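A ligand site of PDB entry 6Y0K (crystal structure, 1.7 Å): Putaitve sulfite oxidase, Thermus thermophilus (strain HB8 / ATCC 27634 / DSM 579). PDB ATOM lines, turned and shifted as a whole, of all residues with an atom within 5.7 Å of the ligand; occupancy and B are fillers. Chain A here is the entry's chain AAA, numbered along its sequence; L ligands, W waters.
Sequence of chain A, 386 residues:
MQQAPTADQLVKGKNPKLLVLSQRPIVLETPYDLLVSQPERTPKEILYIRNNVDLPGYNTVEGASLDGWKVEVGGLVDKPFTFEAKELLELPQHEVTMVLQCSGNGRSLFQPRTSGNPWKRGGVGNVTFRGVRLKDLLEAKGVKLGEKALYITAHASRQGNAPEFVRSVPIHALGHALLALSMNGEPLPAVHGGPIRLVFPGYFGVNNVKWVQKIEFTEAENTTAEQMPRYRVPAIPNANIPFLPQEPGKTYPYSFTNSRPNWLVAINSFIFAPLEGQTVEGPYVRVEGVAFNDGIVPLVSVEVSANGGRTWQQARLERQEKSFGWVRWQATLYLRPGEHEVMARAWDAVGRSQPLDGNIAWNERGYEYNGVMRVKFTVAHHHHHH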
ATOM      1  N   LEU A  47      -5.654  -0.971 -17.720  1.00  0.00           N
ATOM      2  CA  LEU A  47      -6.357  -0.762 -19.024  1.00  0.00           C
ATOM      3  C   LEU A  47      -5.863   0.557 -19.644  1.00  0.00           C
ATOM      4  O   LEU A  47      -5.778   1.585 -18.938  1.00  0.00           O
ATOM      5  CB  LEU A  47      -7.861  -0.794 -18.801  1.00  0.00           C
ATOM      6  CG  LEU A  47      -8.752  -0.632 -20.043  1.00  0.00           C
ATOM      7  CD1 LEU A  47      -8.523  -1.759 -21.054  1.00  0.00           C
ATOM      8  CD2 LEU A  47     -10.205  -0.575 -19.624  1.00  0.00           C
ATOM      9  N   TYR A  48      -5.533   0.537 -20.941  1.00  0.00           N
ATOM     10  CA  TYR A  48      -5.056   1.717 -21.702  1.00  0.00           C
ATOM     11  C   TYR A  48      -6.119   2.827 -21.645  1.00  0.00           C
ATOM     12  O   TYR A  48      -7.346   2.569 -21.479  1.00  0.00           O
ATOM     13  CB  TYR A  48      -4.686   1.366 -23.148  1.00  0.00           C
ATOM     14  CG  TYR A  48      -5.864   1.383 -24.094  1.00  0.00           C
ATOM     15  CD1 TYR A  48      -6.710   0.292 -24.233  1.00  0.00           C
ATOM     16  CD2 TYR A  48      -6.143   2.505 -24.862  1.00  0.00           C
ATOM     17  CE1 TYR A  48      -7.803   0.318 -25.077  1.00  0.00           C
ATOM     18  CE2 TYR A  48      -7.235   2.536 -25.714  1.00  0.00           C
ATOM     19  CZ  TYR A  48      -8.053   1.444 -25.849  1.00  0.00           C
ATOM     20  OH  TYR A  48      -9.148   1.494 -26.678  1.00  0.00           O
ATOM     21  N   ILE A  49      -5.661   4.075 -21.775  1.00  0.00           N
ATOM     22  CA  ILE A  49      -6.526   5.267 -21.899  1.00  0.00           C
ATOM     23  C   ILE A  49      -6.188   5.963 -23.211  1.00  0.00           C
ATOM     24  O   ILE A  49      -4.996   6.194 -23.484  1.00  0.00           O
ATOM     25  CB  ILE A  49      -6.350   6.262 -20.734  1.00  0.00           C
ATOM     26  CG1 ILE A  49      -6.705   5.619 -19.402  1.00  0.00           C
ATOM     27  CG2 ILE A  49      -7.169   7.521 -21.024  1.00  0.00           C
ATOM     28  CD1 ILE A  49      -6.351   6.490 -18.242  1.00  0.00           C
ATOM     29  N   ARG A  50      -7.220   6.351 -23.955  1.00  0.00           N
ATOM     30  CA  ARG A  50      -7.077   7.348 -25.041  1.00  0.00           C
ATOM     31  C   ARG A  50      -8.260   8.311 -24.953  1.00  0.00           C
ATOM     32  O   ARG A  50      -9.376   7.919 -25.315  1.00  0.00           O
ATOM     33  CB  ARG A  50      -6.969   6.704 -26.417  1.00  0.00           C
ATOM     34  CG  ARG A  50      -6.370   7.602 -27.498  1.00  0.00           C
ATOM     35  CD  ARG A  50      -7.202   8.850 -27.797  1.00  0.00           C
ATOM     36  NE  ARG A  50      -6.809   9.378 -29.102  1.00  0.00           N
ATOM     37  CZ  ARG A  50      -6.244  10.556 -29.334  1.00  0.00           C
ATOM     38  NH1 ARG A  50      -5.991  11.403 -28.361  1.00  0.00           N
ATOM     39  NH2 ARG A  50      -5.913  10.874 -30.568  1.00  0.00           N
ATOM     40  N   ASN A  51      -8.010   9.497 -24.434  1.00  0.00           N
ATOM     41  CA  ASN A  51      -8.926  10.648 -24.605  1.00  0.00           C
ATOM     42  C   ASN A  51      -8.475  11.497 -25.800  1.00  0.00           C
ATOM     43  O   ASN A  51      -7.286  11.836 -25.846  1.00  0.00           O
ATOM     44  CB  ASN A  51      -8.940  11.522 -23.366  1.00  0.00           C
ATOM     45  CG  ASN A  51      -9.657  10.871 -22.202  1.00  0.00           C
ATOM     46  OD1 ASN A  51     -10.394   9.908 -22.397  1.00  0.00           O
ATOM     47  ND2 ASN A  51      -9.439  11.405 -21.005  1.00  0.00           N
ATOM     48  N   ASN A  52      -9.392  11.836 -26.703  1.00  0.00           N
ATOM     49  CA  ASN A  52      -9.228  12.997 -27.619  1.00  0.00           C
ATOM     50  C   ASN A  52      -9.574  14.266 -26.834  1.00  0.00           C
ATOM     51  O   ASN A  52      -8.914  15.300 -27.037  1.00  0.00           O
ATOM     52  CB  ASN A  52     -10.160  12.929 -28.836  1.00  0.00           C
ATOM     53  CG  ASN A  52      -9.682  11.947 -29.883  1.00  0.00           C
ATOM     54  OD1 ASN A  52      -8.914  12.337 -30.777  1.00  0.00           O
ATOM     55  ND2 ASN A  52     -10.129  10.710 -29.781  1.00  0.00           N
ATOM     56  N   VAL A  53     -10.591  14.168 -25.981  1.00  0.00           N
ATOM     57  CA  VAL A  53     -11.076  15.336 -25.174  1.00  0.00           C
ATOM     58  C   VAL A  53     -11.217  14.857 -23.728  1.00  0.00           C
ATOM     59  O   VAL A  53     -12.061  13.990 -23.480  1.00  0.00           O
ATOM     60  CB  VAL A  53     -12.411  15.906 -25.690  1.00  0.00           C
ATOM     61  CG1 VAL A  53     -12.882  17.071 -24.835  1.00  0.00           C
ATOM     62  CG2 VAL A  53     -12.332  16.299 -27.153  1.00  0.00           C
ATOM     63  N   ASP A  54     -10.390  15.397 -22.845  1.00  0.00           N
ATOM     64  CA  ASP A  54     -10.468  15.155 -21.379  1.00  0.00           C
ATOM     65  C   ASP A  54     -11.746  15.814 -20.854  1.00  0.00           C
ATOM     66  O   ASP A  54     -12.004  16.976 -21.220  1.00  0.00           O
ATOM     67  CB  ASP A  54      -9.229  15.710 -20.677  1.00  0.00           C
ATOM     68  CG  ASP A  54      -7.904  15.062 -21.031  1.00  0.00           C
ATOM     69  OD1 ASP A  54      -7.887  13.905 -21.468  1.00  0.00           O
ATOM     70  OD2 ASP A  54      -6.864  15.753 -20.871  1.00  0.00           O
ATOM     71  N   LEU A 100     -11.673  -3.979 -26.333  1.00  0.00           N
ATOM     72  CA  LEU A 100     -11.654  -2.506 -26.479  1.00  0.00           C
ATOM     73  C   LEU A 100     -10.269  -2.181 -27.046  1.00  0.00           C
ATOM     74  O   LEU A 100      -9.270  -2.368 -26.357  1.00  0.00           O
ATOM     75  CB  LEU A 100     -11.895  -1.855 -25.119  1.00  0.00           C
ATOM     76  CG  LEU A 100     -11.954  -0.334 -25.113  1.00  0.00           C
ATOM     77  CD1 LEU A 100     -13.170   0.135 -25.916  1.00  0.00           C
ATOM     78  CD2 LEU A 100     -11.992   0.191 -23.685  1.00  0.00           C
ATOM     79  N   GLN A 101     -10.204  -1.826 -28.320  1.00  0.00           N
ATOM     80  CA  GLN A 101      -8.924  -1.596 -29.001  1.00  0.00           C
ATOM     81  C   GLN A 101      -8.946  -0.220 -29.660  1.00  0.00           C
ATOM     82  O   GLN A 101      -9.895   0.069 -30.396  1.00  0.00           O
ATOM     83  CB  GLN A 101      -8.636  -2.640 -30.068  1.00  0.00           C
ATOM     84  CG  GLN A 101      -7.211  -2.492 -30.576  1.00  0.00           C
ATOM     85  CD  GLN A 101      -6.764  -3.541 -31.562  1.00  0.00           C
ATOM     86  OE1 GLN A 101      -5.574  -3.846 -31.654  1.00  0.00           O
ATOM     87  NE2 GLN A 101      -7.706  -4.075 -32.339  1.00  0.00           N
ATOM     88  N   CYS A 102      -7.895   0.553 -29.469  1.00  0.00           N
ATOM     89  CA  CYS A 102      -7.763   1.868 -30.157  1.00  0.00           C
ATOM     90  C   CYS A 102      -7.591   1.616 -31.665  1.00  0.00           C
ATOM     91  O   CYS A 102      -6.855   0.666 -32.016  1.00  0.00           O
ATOM     92  CB  CYS A 102      -6.618   2.641 -29.532  1.00  0.00           C
ATOM     93  SG  CYS A 102      -6.383   4.302 -30.221  1.00  0.00           S
ATOM     94  N   SER A 103      -8.254   2.399 -32.519  1.00  0.00           N
ATOM     95  CA  SER A 103      -8.026   2.401 -33.997  1.00  0.00           C
ATOM     96  C   SER A 103      -6.520   2.413 -34.280  1.00  0.00           C
ATOM     97  O   SER A 103      -6.065   1.811 -35.240  1.00  0.00           O
ATOM     98  CB  SER A 103      -8.703   3.615 -34.632  1.00  0.00           C
ATOM     99  OG  SER A 103     -10.071   3.680 -34.254  1.00  0.00           O
ATOM    100  N   GLY A 104      -5.752   3.148 -33.472  1.00  0.00           N
ATOM    101  CA  GLY A 104      -4.323   3.359 -33.709  1.00  0.00           C
ATOM    102  C   GLY A 104      -3.449   2.286 -33.097  1.00  0.00           C
ATOM    103  O   GLY A 104      -2.235   2.370 -33.281  1.00  0.00           O
ATOM    104  N   TRP A 119       1.498   4.040 -30.387  1.00  0.00           N
ATOM    105  CA  TRP A 119       1.169   2.705 -29.825  1.00  0.00           C
ATOM    106  C   TRP A 119       2.132   1.644 -30.370  1.00  0.00           C
ATOM    107  O   TRP A 119       2.469   1.698 -31.558  1.00  0.00           O
ATOM    108  CB  TRP A 119      -0.270   2.301 -30.171  1.00  0.00           C
ATOM    109  CG  TRP A 119      -1.345   3.260 -29.746  1.00  0.00           C
ATOM    110  CD1 TRP A 119      -2.042   4.096 -30.557  1.00  0.00           C
ATOM    111  CD2 TRP A 119      -1.864   3.463 -28.418  1.00  0.00           C
ATOM    112  NE1 TRP A 119      -2.955   4.805 -29.836  1.00  0.00           N
ATOM    113  CE2 TRP A 119      -2.876   4.444 -28.521  1.00  0.00           C
ATOM    114  CE3 TRP A 119      -1.585   2.929 -27.160  1.00  0.00           C
ATOM    115  CZ2 TRP A 119      -3.596   4.883 -27.418  1.00  0.00           C
ATOM    116  CZ3 TRP A 119      -2.297   3.367 -26.069  1.00  0.00           C
ATOM    117  CH2 TRP A 119      -3.284   4.342 -26.197  1.00  0.00           C
ATOM    118  N   ALA A 156     -20.568  13.115 -26.863  1.00  0.00           N
ATOM    119  CA  ALA A 156     -20.089  13.219 -25.473  1.00  0.00           C
ATOM    120  C   ALA A 156     -20.604  14.493 -24.795  1.00  0.00           C
ATOM    121  O   ALA A 156     -20.949  15.504 -25.464  1.00  0.00           O
ATOM    122  CB  ALA A 156     -18.591  13.181 -25.454  1.00  0.00           C
ATOM    123  N   PHE A 165     -17.267  15.758 -28.930  1.00  0.00           N
ATOM    124  CA  PHE A 165     -16.771  14.458 -29.423  1.00  0.00           C
ATOM    125  C   PHE A 165     -17.977  13.686 -29.926  1.00  0.00           C
ATOM    126  O   PHE A 165     -18.839  13.276 -29.131  1.00  0.00           O
ATOM    127  CB  PHE A 165     -15.988  13.694 -28.360  1.00  0.00           C
ATOM    128  CG  PHE A 165     -15.304  12.497 -28.963  1.00  0.00           C
ATOM    129  CD1 PHE A 165     -14.118  12.647 -29.649  1.00  0.00           C
ATOM    130  CD2 PHE A 165     -15.889  11.254 -28.896  1.00  0.00           C
ATOM    131  CE1 PHE A 165     -13.507  11.549 -30.235  1.00  0.00           C
ATOM    132  CE2 PHE A 165     -15.278  10.157 -29.482  1.00  0.00           C
ATOM    133  CZ  PHE A 165     -14.094  10.313 -30.152  1.00  0.00           C
ATOM    134  N   VAL A 191     -12.600   7.717 -15.762  1.00  0.00           N
ATOM    135  CA  VAL A 191     -11.618   7.904 -16.864  1.00  0.00           C
ATOM    136  C   VAL A 191     -11.960   6.996 -18.057  1.00  0.00           C
ATOM    137  O   VAL A 191     -11.476   7.283 -19.169  1.00  0.00           O
ATOM    138  CB  VAL A 191     -10.168   7.689 -16.377  1.00  0.00           C
ATOM    139  CG1 VAL A 191      -9.842   6.209 -16.148  1.00  0.00           C
ATOM    140  CG2 VAL A 191      -9.201   8.344 -17.345  1.00  0.00           C
ATOM    141  N   HIS A 192     -12.750   5.948 -17.847  1.00  0.00           N
ATOM    142  CA  HIS A 192     -13.213   5.008 -18.900  1.00  0.00           C
ATOM    143  C   HIS A 192     -14.643   5.364 -19.316  1.00  0.00           C
ATOM    144  O   HIS A 192     -15.292   4.525 -19.970  1.00  0.00           O
ATOM    145  CB  HIS A 192     -13.032   3.550 -18.461  1.00  0.00           C
ATOM    146  CG  HIS A 192     -11.605   3.175 -18.371  1.00  0.00           C
ATOM    147  ND1 HIS A 192     -10.780   3.121 -19.484  1.00  0.00           N
ATOM    148  CD2 HIS A 192     -10.812   2.885 -17.298  1.00  0.00           C
ATOM    149  CE1 HIS A 192      -9.553   2.807 -19.095  1.00  0.00           C
ATOM    150  NE2 HIS A 192      -9.546   2.650 -17.766  1.00  0.00           N
ATOM    151  N   GLY A 193     -15.135   6.544 -18.911  1.00  0.00           N
ATOM    152  CA  GLY A 193     -16.410   7.126 -19.397  1.00  0.00           C
ATOM    153  C   GLY A 193     -17.540   7.052 -18.401  1.00  0.00           C
ATOM    154  O   GLY A 193     -18.679   7.412 -18.758  1.00  0.00           O
ATOM    155  N   ARG A 197     -21.373   5.232 -20.663  1.00  0.00           N
ATOM    156  CA  ARG A 197     -20.646   5.132 -21.941  1.00  0.00           C
ATOM    157  C   ARG A 197     -21.491   4.328 -22.914  1.00  0.00           C
ATOM    158  O   ARG A 197     -22.043   3.290 -22.518  1.00  0.00           O
ATOM    159  CB  ARG A 197     -19.296   4.481 -21.680  1.00  0.00           C
ATOM    160  CG  ARG A 197     -18.438   4.352 -22.934  1.00  0.00           C
ATOM    161  CD  ARG A 197     -17.083   3.791 -22.602  1.00  0.00           C
ATOM    162  NE  ARG A 197     -16.144   3.956 -23.700  1.00  0.00           N
ATOM    163  CZ  ARG A 197     -14.829   3.790 -23.611  1.00  0.00           C
ATOM    164  NH1 ARG A 197     -14.284   3.392 -22.466  1.00  0.00           N
ATOM    165  NH2 ARG A 197     -14.061   3.988 -24.665  1.00  0.00           N
ATOM    166  N   PHE A 204     -14.141  -0.419 -33.128  1.00  0.00           N
ATOM    167  CA  PHE A 204     -12.929   0.222 -32.578  1.00  0.00           C
ATOM    168  C   PHE A 204     -13.300   1.234 -31.484  1.00  0.00           C
ATOM    169  O   PHE A 204     -14.388   1.810 -31.489  1.00  0.00           O
ATOM    170  CB  PHE A 204     -12.107   0.862 -33.686  1.00  0.00           C
ATOM    171  CG  PHE A 204     -11.172  -0.061 -34.422  1.00  0.00           C
ATOM    172  CD1 PHE A 204     -10.039  -0.571 -33.790  1.00  0.00           C
ATOM    173  CD2 PHE A 204     -11.385  -0.398 -35.742  1.00  0.00           C
ATOM    174  CE1 PHE A 204      -9.168  -1.399 -34.474  1.00  0.00           C
ATOM    175  CE2 PHE A 204     -10.507  -1.232 -36.429  1.00  0.00           C
ATOM    176  CZ  PHE A 204      -9.402  -1.730 -35.793  1.00  0.00           C
ATOM    177  N   GLY A 205     -12.356   1.411 -30.542  1.00  0.00           N
ATOM    178  CA  GLY A 205     -12.491   2.205 -29.313  1.00  0.00           C
ATOM    179  C   GLY A 205     -13.053   3.591 -29.543  1.00  0.00           C
ATOM    180  O   GLY A 205     -13.911   3.977 -28.772  1.00  0.00           O
ATOM    181  N   VAL A 206     -12.597   4.273 -30.582  1.00  0.00           N
ATOM    182  CA  VAL A 206     -13.043   5.658 -30.927  1.00  0.00           C
ATOM    183  C   VAL A 206     -14.561   5.763 -30.894  1.00  0.00           C
ATOM    184  O   VAL A 206     -15.095   6.824 -30.453  1.00  0.00           O
ATOM    185  CB  VAL A 206     -12.459   6.124 -32.268  1.00  0.00           C
ATOM    186  CG1 VAL A 206     -13.000   5.341 -33.470  1.00  0.00           C
ATOM    187  CG2 VAL A 206     -12.722   7.623 -32.439  1.00  0.00           C
ATOM    188  N   ASN A 207     -15.276   4.731 -31.347  1.00  0.00           N
ATOM    189  CA  ASN A 207     -16.761   4.742 -31.454  1.00  0.00           C
ATOM    190  C   ASN A 207     -17.473   4.609 -30.097  1.00  0.00           C
ATOM    191  O   ASN A 207     -18.690   4.871 -30.062  1.00  0.00           O
ATOM    192  CB  ASN A 207     -17.218   3.612 -32.365  1.00  0.00           C
ATOM    193  CG  ASN A 207     -16.571   3.764 -33.720  1.00  0.00           C
ATOM    194  OD1 ASN A 207     -16.825   4.755 -34.424  1.00  0.00           O
ATOM    195  ND2 ASN A 207     -15.700   2.829 -34.064  1.00  0.00           N
ATOM    196  N   ASN A 208     -16.789   4.122 -29.073  1.00  0.00           N
ATOM    197  CA  ASN A 208     -17.375   3.812 -27.752  1.00  0.00           C
ATOM    198  C   ASN A 208     -17.325   5.112 -26.936  1.00  0.00           C
ATOM    199  O   ASN A 208     -16.330   5.329 -26.237  1.00  0.00           O
ATOM    200  CB  ASN A 208     -16.650   2.621 -27.107  1.00  0.00           C
ATOM    201  CG  ASN A 208     -16.785   1.351 -27.928  1.00  0.00           C
ATOM    202  OD1 ASN A 208     -17.754   0.643 -27.788  1.00  0.00           O
ATOM    203  ND2 ASN A 208     -15.832   1.045 -28.801  1.00  0.00           N
ATOM    204  N   VAL A 209     -18.362   5.947 -27.078  1.00  0.00           N
ATOM    205  CA  VAL A 209     -18.338   7.360 -26.613  1.00  0.00           C
ATOM    206  C   VAL A 209     -18.512   7.409 -25.105  1.00  0.00           C
ATOM    207  O   VAL A 209     -19.587   7.088 -24.609  1.00  0.00           O
ATOM    208  CB  VAL A 209     -19.366   8.221 -27.362  1.00  0.00           C
ATOM    209  CG1 VAL A 209     -19.411   9.623 -26.770  1.00  0.00           C
ATOM    210  CG2 VAL A 209     -19.051   8.269 -28.846  1.00  0.00           C
ATOM    211  N   LYS A 210     -17.452   7.845 -24.410  1.00  0.00           N
ATOM    212  CA  LYS A 210     -17.431   8.081 -22.956  1.00  0.00           C
ATOM    213  C   LYS A 210     -18.342   9.248 -22.611  1.00  0.00           C
ATOM    214  O   LYS A 210     -18.505  10.167 -23.457  1.00  0.00           O
ATOM    215  CB  LYS A 210     -16.012   8.419 -22.523  1.00  0.00           C
ATOM    216  CG  LYS A 210     -14.956   7.353 -22.769  1.00  0.00           C
ATOM    217  CD  LYS A 210     -13.612   7.850 -22.305  1.00  0.00           C
ATOM    218  CE  LYS A 210     -12.488   6.901 -22.621  1.00  0.00           C
ATOM    219  NZ  LYS A 210     -11.217   7.349 -21.995  1.00  0.00           N
ATOM    220  N   TRP A 211     -18.954   9.243 -21.444  1.00  0.00           N
ATOM    221  CA  TRP A 211     -19.741  10.398 -20.920  1.00  0.00           C
ATOM    222  C   TRP A 211     -20.852  10.753 -21.913  1.00  0.00           C
ATOM    223  O   TRP A 211     -21.053  11.968 -22.236  1.00  0.00           O
ATOM    224  CB  TRP A 211     -18.801  11.570 -20.631  1.00  0.00           C
ATOM    225  CG  TRP A 211     -17.561  11.161 -19.893  1.00  0.00           C
ATOM    226  CD1 TRP A 211     -17.498  10.530 -18.683  1.00  0.00           C
ATOM    227  CD2 TRP A 211     -16.206  11.272 -20.363  1.00  0.00           C
ATOM    228  NE1 TRP A 211     -16.195  10.247 -18.371  1.00  0.00           N
ATOM    229  CE2 TRP A 211     -15.377  10.725 -19.357  1.00  0.00           C
ATOM    230  CE3 TRP A 211     -15.600  11.809 -21.510  1.00  0.00           C
ATOM    231  CZ2 TRP A 211     -13.994  10.647 -19.488  1.00  0.00           C
ATOM    232  CZ3 TRP A 211     -14.227  11.761 -21.624  1.00  0.00           C
ATOM    233  CH2 TRP A 211     -13.434  11.203 -20.618  1.00  0.00           C
ATOM    234  N   TYR A 231      -9.864   9.271 -38.331  1.00  0.00           N
ATOM    235  CA  TYR A 231     -10.462   7.934 -38.027  1.00  0.00           C
ATOM    236  C   TYR A 231     -11.071   7.340 -39.286  1.00  0.00           C
ATOM    237  O   TYR A 231     -12.172   6.735 -39.219  1.00  0.00           O
ATOM    238  CB  TYR A 231     -11.444   8.051 -36.861  1.00  0.00           C
ATOM    239  CG  TYR A 231     -10.753   8.424 -35.589  1.00  0.00           C
ATOM    240  CD1 TYR A 231      -9.899   7.525 -34.976  1.00  0.00           C
ATOM    241  CD2 TYR A 231     -10.903   9.670 -35.019  1.00  0.00           C
ATOM    242  CE1 TYR A 231      -9.219   7.859 -33.828  1.00  0.00           C
ATOM    243  CE2 TYR A 231     -10.248  10.012 -33.845  1.00  0.00           C
ATOM    244  CZ  TYR A 231      -9.368   9.110 -33.265  1.00  0.00           C
ATOM    245  OH  TYR A 231      -8.686   9.420 -32.132  1.00  0.00           O
ATOM    246  N   ASN A 262     -13.103   4.035 -39.165  1.00  0.00           N
ATOM    247  CA  ASN A 262     -12.696   2.965 -38.237  1.00  0.00           C
ATOM    248  C   ASN A 262     -13.949   2.494 -37.505  1.00  0.00           C
ATOM    249  O   ASN A 262     -14.416   3.193 -36.604  1.00  0.00           O
ATOM    250  CB  ASN A 262     -11.643   3.419 -37.243  1.00  0.00           C
ATOM    251  CG  ASN A 262     -10.426   4.057 -37.860  1.00  0.00           C
ATOM    252  OD1 ASN A 262      -9.929   5.011 -37.287  1.00  0.00           O
ATOM    253  ND2 ASN A 262      -9.917   3.550 -38.990  1.00  0.00           N
HETATM  254  N1  LIG L   1     -15.170   9.163 -25.784  1.00  0.00           N
HETATM  255  C1  LIG L   1     -15.133  10.515 -25.513  1.00  0.00           C
HETATM  256  N2  LIG L   1     -16.223  11.119 -25.008  1.00  0.00           N
HETATM  257  N3  LIG L   1     -14.043  11.298 -25.742  1.00  0.00           N
HETATM  258  C2  LIG L   1     -12.900  10.820 -26.266  1.00  0.00           C
HETATM  259  O1  LIG L   1     -11.924  11.572 -26.449  1.00  0.00           O
HETATM  260  N4  LIG L   1     -11.733   8.771 -27.146  1.00  0.00           N
HETATM  261  C3  LIG L   1     -12.046   7.575 -27.922  1.00  0.00           C
HETATM  262  C4  LIG L   1     -13.004   6.621 -27.183  1.00  0.00           C
HETATM  263  N5  LIG L   1     -14.093   7.293 -26.573  1.00  0.00           N
HETATM  264  C5  LIG L   1     -12.814   9.379 -26.553  1.00  0.00           C
HETATM  265  C6  LIG L   1     -14.065   8.599 -26.297  1.00  0.00           C
HETATM  266  C7  LIG L   1     -10.842   6.780 -28.390  1.00  0.00           C
HETATM  267  S1  LIG L   1      -9.866   7.359 -29.671  1.00  0.00           S
HETATM  268  C8  LIG L   1     -10.574   5.563 -27.842  1.00  0.00           C
HETATM  269  S2  LIG L   1      -9.378   4.548 -28.467  1.00  0.00           S
HETATM  270  C9  LIG L   1     -11.331   5.059 -26.636  1.00  0.00           C
HETATM  271  O2  LIG L   1     -12.314   5.961 -26.162  1.00  0.00           O
HETATM  272  C10 LIG L   1     -10.393   4.696 -25.482  1.00  0.00           C
HETATM  273  O3  LIG L   1     -11.150   4.082 -24.432  1.00  0.00           O
HETATM  274  P1  LIG L   1     -10.431   3.977 -22.986  1.00  0.00           P
HETATM  275  O4  LIG L   1      -9.491   2.772 -23.135  1.00  0.00           O
HETATM  276  O5  LIG L   1      -9.667   5.276 -22.761  1.00  0.00           O
HETATM  277  O6  LIG L   1     -11.592   3.740 -22.040  1.00  0.00           O
HETATM  278 MO1  LIG L   1      -8.550   5.573 -30.429  1.00  0.00          MO
HETATM  279  O7  LIG L   1      -9.552   4.789 -31.797  1.00  0.00           O
HETATM  280  O   HOH W   1     -15.113  13.840 -24.516  1.00  0.00           O
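A sulfur (S1) of the ligand sits close to the side-chain hydroxyl (OH) of Tyr 231 (3.4 Å).
N of Asn 52 sits at hydrogen-bond distance from O1 of the ligand, 2.6 Å away.
OH of Tyr 48 lies close to S2 of the ligand (3.5 Å).
A nitrogen (N5) of the ligand sits at hydrogen-bond distance from the backbone carbonyl oxygen (O) of Asn 208, at 3.0 Å.
O of Arg 50 is in hydrogen-bond range of N4 of the ligand (3.1 Å).
O of Lys 210 is in hydrogen-bond range of N2 of the ligand, at 2.9 Å.
The side-chain amino group of Lys 210 is in salt-bridge range of an oxygen (O5) of the ligand.
The backbone carbonyl oxygen of Tyr 48 lies close to an oxygen (O4) of the ligand, 2.7 Å away.
ND1 of His 192 lies within hydrogen-bond range of O6 of the ligand (2.8 Å).
MO1 of the ligand is bound by SG of Cys 102 (2.5 Å).
The side-chain hydroxyl (OG) of Ser 103 sits close to an oxygen (O7) of the ligand (2.7 Å).
The backbone NH (N) of Lys 210 sits at hydrogen-bond distance from a nitrogen (N1) of the ligand, at 3.0 Å.
The guanidinium group of Arg 197 lies within salt-bridge range of an oxygen (O6) of the ligand.
An oxygen (O1) of the ligand lies within hydrogen-bond range of the backbone NH of Val 53, at 3.0 Å.
ND2 of Asn 52 sits close to S1 of the ligand (3.4 Å).
An oxygen (O5) of the ligand lies within hydrogen-bond range of the backbone NH (N) of Arg 50 (2.9 Å).
A sulfur (S1) of the ligand lies close to the guanidinium group of Arg 50 (3.7 Å).
The side-chain carboxylate (OD1) of Asp 54 sits at hydrogen-bond distance from the side-chain amide nitrogen (ND2) of Asn 51, 3.0 Å away.
The side-chain sulfur of Cys 102 lies close to the backbone NH of Gly 104, 3.5 Å away.
N of Trp 211 is in hydrogen-bond range of O of Gly 193 (3.3 Å).
The indole nitrogen (NE1) of Trp 119 sits close to the side-chain sulfur (SG) of Cys 102 (3.5 Å).
N of Cys 102 sits at hydrogen-bond distance from OH of Tyr 48 (3.2 Å).
The side-chain amino group of Lys 210 is in hydrogen-bond range of the side-chain amide oxygen of Asn 51, at 2.7 Å.
The guanidinium group of Arg 197 lies within hydrogen-bond range of the backbone carbonyl oxygen of Asn 208, at 2.9 Å.
ND2 of Asn 208 sits at hydrogen-bond distance from O of Phe 204 (3.1 Å).
O7 of the ligand sits close to N of Val 206 (3.3 Å).
Ile 49 touches the ligand.
C of Asn 51 touches O1 of the ligand (3.5 Å).
CD2 of Leu 100 touches O4 of the ligand, at 3.6 Å.
Ala 156 touches the ligand.
Phe 165 touches the ligand.
Gly 205 touches the ligand.
CA of Val 209 touches N1 of the ligand, 3.7 Å away.
Trp 211 touches the ligand.
Hydrophobic or aromatic side chains within 4 Å of the ligand: Tyr 48, Ile 49, Leu 100, Ala 156, Phe 165, His 192, Val 206, Val 209, Trp 211 and Tyr 231.
The nearest printed residue that does not touch the ligand is Gly 104 (4.5 Å).
Water W1 lies within hydrogen-bond range of a nitrogen (N2) of the ligand and the backbone carbonyl oxygen (O) of Val 53.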
